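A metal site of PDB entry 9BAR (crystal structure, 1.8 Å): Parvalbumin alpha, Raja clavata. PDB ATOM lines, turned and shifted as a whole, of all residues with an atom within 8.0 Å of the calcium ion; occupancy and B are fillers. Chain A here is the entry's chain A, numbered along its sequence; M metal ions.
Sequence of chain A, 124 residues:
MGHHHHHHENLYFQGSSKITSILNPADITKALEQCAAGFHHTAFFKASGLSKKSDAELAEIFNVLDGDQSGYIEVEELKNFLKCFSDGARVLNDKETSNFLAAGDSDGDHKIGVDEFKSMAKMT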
ATOM      1  N   PHE A  62      -0.564 -27.040  14.581  1.00  0.00           N
ATOM      2  CA  PHE A  62       0.757 -26.473  14.696  1.00  0.00           C
ATOM      3  C   PHE A  62       1.229 -26.513  16.149  1.00  0.00           C
ATOM      4  O   PHE A  62       2.377 -26.868  16.412  1.00  0.00           O
ATOM      5  CB  PHE A  62       0.746 -25.021  14.198  1.00  0.00           C
ATOM      6  CG  PHE A  62       2.077 -24.315  14.391  1.00  0.00           C
ATOM      7  CD1 PHE A  62       3.076 -24.437  13.440  1.00  0.00           C
ATOM      8  CD2 PHE A  62       2.310 -23.550  15.522  1.00  0.00           C
ATOM      9  CE1 PHE A  62       4.294 -23.808  13.629  1.00  0.00           C
ATOM     10  CE2 PHE A  62       3.528 -22.905  15.692  1.00  0.00           C
ATOM     11  CZ  PHE A  62       4.515 -23.037  14.760  1.00  0.00           C
ATOM     12  N   ASN A  63       0.353 -26.131  17.081  1.00  0.00           N
ATOM     13  CA  ASN A  63       0.720 -26.073  18.489  1.00  0.00           C
ATOM     14  C   ASN A  63       1.066 -27.453  19.043  1.00  0.00           C
ATOM     15  O   ASN A  63       1.889 -27.562  19.934  1.00  0.00           O
ATOM     16  CB  ASN A  63      -0.350 -25.408  19.331  1.00  0.00           C
ATOM     17  CG  ASN A  63      -0.437 -23.943  18.993  1.00  0.00           C
ATOM     18  OD1 ASN A  63       0.604 -23.309  18.733  1.00  0.00           O
ATOM     19  ND2 ASN A  63      -1.632 -23.408  18.926  1.00  0.00           N
ATOM     20  N   LEU A  65       2.353 -29.982  17.122  1.00  0.00           N
ATOM     21  CA  LEU A  65       3.611 -30.304  16.467  1.00  0.00           C
ATOM     22  C   LEU A  65       4.789 -29.599  17.129  1.00  0.00           C
ATOM     23  O   LEU A  65       5.923 -30.094  17.099  1.00  0.00           O
ATOM     24  CB  LEU A  65       3.546 -29.920  14.989  1.00  0.00           C
ATOM     25  CG  LEU A  65       2.452 -30.582  14.150  1.00  0.00           C
ATOM     26  CD1 LEU A  65       2.420 -30.055  12.731  1.00  0.00           C
ATOM     27  CD2 LEU A  65       2.607 -32.083  14.148  1.00  0.00           C
ATOM     28  N   ASP A  66       4.560 -28.378  17.625  1.00  0.00           N
ATOM     29  CA  ASP A  66       5.560 -27.607  18.343  1.00  0.00           C
ATOM     30  C   ASP A  66       5.724 -28.166  19.758  1.00  0.00           C
ATOM     31  O   ASP A  66       5.202 -27.596  20.719  1.00  0.00           O
ATOM     32  CB  ASP A  66       5.180 -26.141  18.313  1.00  0.00           C
ATOM     33  CG  ASP A  66       6.161 -25.181  18.966  1.00  0.00           C
ATOM     34  OD1 ASP A  66       7.326 -25.586  19.203  1.00  0.00           O
ATOM     35  OD2 ASP A  66       5.760 -24.021  19.204  1.00  0.00           O
ATOM     36  N   GLY A  67       6.470 -29.266  19.875  1.00  0.00           N
ATOM     37  CA  GLY A  67       6.628 -30.039  21.100  1.00  0.00           C
ATOM     38  C   GLY A  67       7.181 -29.253  22.291  1.00  0.00           C
ATOM     39  O   GLY A  67       6.860 -29.585  23.427  1.00  0.00           O
ATOM     40  N   ASP A  68       8.043 -28.255  22.045  1.00  0.00           N
ATOM     41  CA  ASP A  68       8.707 -27.493  23.097  1.00  0.00           C
ATOM     42  C   ASP A  68       8.081 -26.100  23.241  1.00  0.00           C
ATOM     43  O   ASP A  68       8.607 -25.266  23.973  1.00  0.00           O
ATOM     44  CB  ASP A  68      10.197 -27.379  22.846  1.00  0.00           C
ATOM     45  CG  ASP A  68      10.620 -26.519  21.658  1.00  0.00           C
ATOM     46  OD1 ASP A  68       9.763 -26.227  20.799  1.00  0.00           O
ATOM     47  OD2 ASP A  68      11.809 -26.137  21.598  1.00  0.00           O
ATOM     48  N   GLN A  69       6.983 -25.853  22.530  1.00  0.00           N
ATOM     49  CA  GLN A  69       6.281 -24.573  22.530  1.00  0.00           C
ATOM     50  C   GLN A  69       7.252 -23.400  22.332  1.00  0.00           C
ATOM     51  O   GLN A  69       7.184 -22.387  23.039  1.00  0.00           O
ATOM     52  CB  GLN A  69       5.415 -24.481  23.795  1.00  0.00           C
ATOM     53  CG  GLN A  69       4.321 -25.539  23.830  1.00  0.00           C
ATOM     54  CD  GLN A  69       3.206 -25.279  22.832  1.00  0.00           C
ATOM     55  OE1 GLN A  69       3.011 -26.038  21.860  1.00  0.00           O
ATOM     56  NE2 GLN A  69       2.462 -24.213  23.061  1.00  0.00           N
ATOM     57  N   SER A  70       8.075 -23.497  21.297  1.00  0.00           N
ATOM     58  CA  SER A  70       9.043 -22.463  20.951  1.00  0.00           C
ATOM     59  C   SER A  70       8.404 -21.382  20.090  1.00  0.00           C
ATOM     60  O   SER A  70       8.955 -20.287  19.961  1.00  0.00           O
ATOM     61  CB  SER A  70      10.227 -23.037  20.243  1.00  0.00           C
ATOM     62  OG  SER A  70       9.843 -23.612  18.999  1.00  0.00           O
ATOM     63  N   GLY A  71       7.265 -21.703  19.471  1.00  0.00           N
ATOM     64  CA  GLY A  71       6.663 -20.827  18.484  1.00  0.00           C
ATOM     65  C   GLY A  71       7.017 -21.229  17.060  1.00  0.00           C
ATOM     66  O   GLY A  71       6.481 -20.660  16.104  1.00  0.00           O
ATOM     67  N   TYR A  72       7.899 -22.234  16.917  1.00  0.00           N
ATOM     68  CA  TYR A  72       8.338 -22.711  15.623  1.00  0.00           C
ATOM     69  C   TYR A  72       8.449 -24.224  15.615  1.00  0.00           C
ATOM     70  O   TYR A  72       8.667 -24.835  16.667  1.00  0.00           O
ATOM     71  CB  TYR A  72       9.712 -22.157  15.232  1.00  0.00           C
ATOM     72  CG  TYR A  72       9.825 -20.654  15.431  1.00  0.00           C
ATOM     73  CD1 TYR A  72       9.389 -19.770  14.446  1.00  0.00           C
ATOM     74  CD2 TYR A  72      10.324 -20.130  16.614  1.00  0.00           C
ATOM     75  CE1 TYR A  72       9.476 -18.396  14.645  1.00  0.00           C
ATOM     76  CE2 TYR A  72      10.428 -18.770  16.816  1.00  0.00           C
ATOM     77  CZ  TYR A  72       9.999 -17.907  15.829  1.00  0.00           C
ATOM     78  OH  TYR A  72      10.125 -16.569  16.070  1.00  0.00           O
ATOM     79  N   ILE A  73       8.340 -24.793  14.417  1.00  0.00           N
ATOM     80  CA  ILE A  73       8.785 -26.149  14.162  1.00  0.00           C
ATOM     81  C   ILE A  73      10.211 -26.048  13.648  1.00  0.00           C
ATOM     82  O   ILE A  73      10.425 -25.575  12.526  1.00  0.00           O
ATOM     83  CB  ILE A  73       7.862 -26.872  13.164  1.00  0.00           C
ATOM     84  CG1 ILE A  73       6.404 -26.819  13.633  1.00  0.00           C
ATOM     85  CG2 ILE A  73       8.338 -28.301  12.925  1.00  0.00           C
ATOM     86  CD1 ILE A  73       5.385 -27.176  12.548  1.00  0.00           C
ATOM     87  N   GLU A  74      11.173 -26.418  14.509  1.00  0.00           N
ATOM     88  CA  GLU A  74      12.586 -26.406  14.178  1.00  0.00           C
ATOM     89  C   GLU A  74      12.901 -27.661  13.359  1.00  0.00           C
ATOM     90  O   GLU A  74      12.094 -28.589  13.319  1.00  0.00           O
ATOM     91  CB  GLU A  74      13.455 -26.343  15.441  1.00  0.00           C
ATOM     92  CG  GLU A  74      13.359 -25.027  16.211  1.00  0.00           C
ATOM     93  CD  GLU A  74      12.188 -24.822  17.164  1.00  0.00           C
ATOM     94  OE1 GLU A  74      11.583 -25.812  17.641  1.00  0.00           O
ATOM     95  OE2 GLU A  74      11.876 -23.638  17.448  1.00  0.00           O
ATOM     96  N   VAL A  75      14.078 -27.692  12.707  1.00  0.00           N
ATOM     97  CA  VAL A  75      14.421 -28.777  11.811  1.00  0.00           C
ATOM     98  C   VAL A  75      14.439 -30.102  12.575  1.00  0.00           C
ATOM     99  O   VAL A  75      14.082 -31.143  12.017  1.00  0.00           O
ATOM    100  CB  VAL A  75      15.761 -28.577  11.076  1.00  0.00           C
ATOM    101  CG1 VAL A  75      15.657 -27.498  10.009  1.00  0.00           C
ATOM    102  CG2 VAL A  75      16.894 -28.268  12.043  1.00  0.00           C
ATOM    103  N   GLU A  77      12.564 -30.955  15.038  1.00  0.00           N
ATOM    104  CA  GLU A  77      11.175 -31.374  15.185  1.00  0.00           C
ATOM    105  C   GLU A  77      10.646 -31.905  13.864  1.00  0.00           C
ATOM    106  O   GLU A  77       9.962 -32.923  13.805  1.00  0.00           O
ATOM    107  CB  GLU A  77      10.306 -30.218  15.684  1.00  0.00           C
ATOM    108  CG  GLU A  77      10.591 -29.844  17.139  1.00  0.00           C
ATOM    109  CD  GLU A  77       9.875 -28.604  17.640  1.00  0.00           C
ATOM    110  OE1 GLU A  77       9.560 -27.718  16.819  1.00  0.00           O
ATOM    111  OE2 GLU A  77       9.650 -28.511  18.854  1.00  0.00           O
ATOM    112  N   LEU A  78      11.004 -31.214  12.773  1.00  0.00           N
ATOM    113  CA  LEU A  78      10.523 -31.550  11.447  1.00  0.00           C
ATOM    114  C   LEU A  78      10.971 -32.946  11.052  1.00  0.00           C
ATOM    115  O   LEU A  78      10.228 -33.647  10.387  1.00  0.00           O
ATOM    116  CB  LEU A  78      11.018 -30.470  10.476  1.00  0.00           C
ATOM    117  CG  LEU A  78      10.181 -30.232   9.229  1.00  0.00           C
ATOM    118  CD1 LEU A  78       8.805 -29.706   9.551  1.00  0.00           C
ATOM    119  CD2 LEU A  78      10.945 -29.247   8.353  1.00  0.00           C
ATOM    120  N   LYS A 111      13.131 -22.303  10.010  1.00  0.00           N
ATOM    121  CA  LYS A 111      12.170 -22.946  10.892  1.00  0.00           C
ATOM    122  C   LYS A 111      10.767 -22.611  10.393  1.00  0.00           C
ATOM    123  O   LYS A 111      10.610 -21.717   9.553  1.00  0.00           O
ATOM    124  CB  LYS A 111      12.427 -22.600  12.368  1.00  0.00           C
ATOM    125  CG  LYS A 111      12.671 -21.141  12.693  1.00  0.00           C
ATOM    126  CD  LYS A 111      13.196 -20.971  14.111  1.00  0.00           C
ATOM    127  CE  LYS A 111      13.378 -19.553  14.528  1.00  0.00           C
ATOM    128  NZ  LYS A 111      13.936 -19.497  15.879  1.00  0.00           N
ATOM    129  N   ILE A 112       9.738 -23.336  10.864  1.00  0.00           N
ATOM    130  CA  ILE A 112       8.398 -23.138  10.326  1.00  0.00           C
ATOM    131  C   ILE A 112       7.527 -22.470  11.391  1.00  0.00           C
ATOM    132  O   ILE A 112       7.377 -23.006  12.483  1.00  0.00           O
ATOM    133  CB  ILE A 112       7.784 -24.442   9.786  1.00  0.00           C
ATOM    134  CG1 ILE A 112       8.588 -24.975   8.603  1.00  0.00           C
ATOM    135  CG2 ILE A 112       6.309 -24.245   9.416  1.00  0.00           C
ATOM    136  CD1 ILE A 112       8.118 -26.305   8.065  1.00  0.00           C
HETATM  137 CA    CA M   1       9.458 -25.975  18.521  1.00  0.00          CA
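O of Asp 66 sits close to OE1 of Gln 69 (2.9 Å).
OD2 of Asp 66 is in hydrogen-bond range of N of Gly 71, 2.8 Å away.
The side-chain carboxylate of Glu 77 lies close to the backbone NH of Gly 67 (3.4 Å).
Six residues have an atom within 4 Å of the calcium ion: Asp 66, Asp 68, Ser 70, Tyr 72, Glu 74 and Glu 77.
OD1 of Asp 66 binds the calcium ion (2.3 Å).
The calcium ion is bound by OE1 of Glu 74.
The calcium ion is bound by OD1 of Asp 68, at 2.3 Å.
The calcium ion is bound by O of Tyr 72 (2.3 Å).
OE1 of Glu 77 is bound to the calcium ion (2.4 Å).
OG of Ser 70 is bound to the calcium ion, at 2.4 Å.
OE2 of Glu 77 binds the calcium ion.
The calcium ion has seven donor atoms within binding distance.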
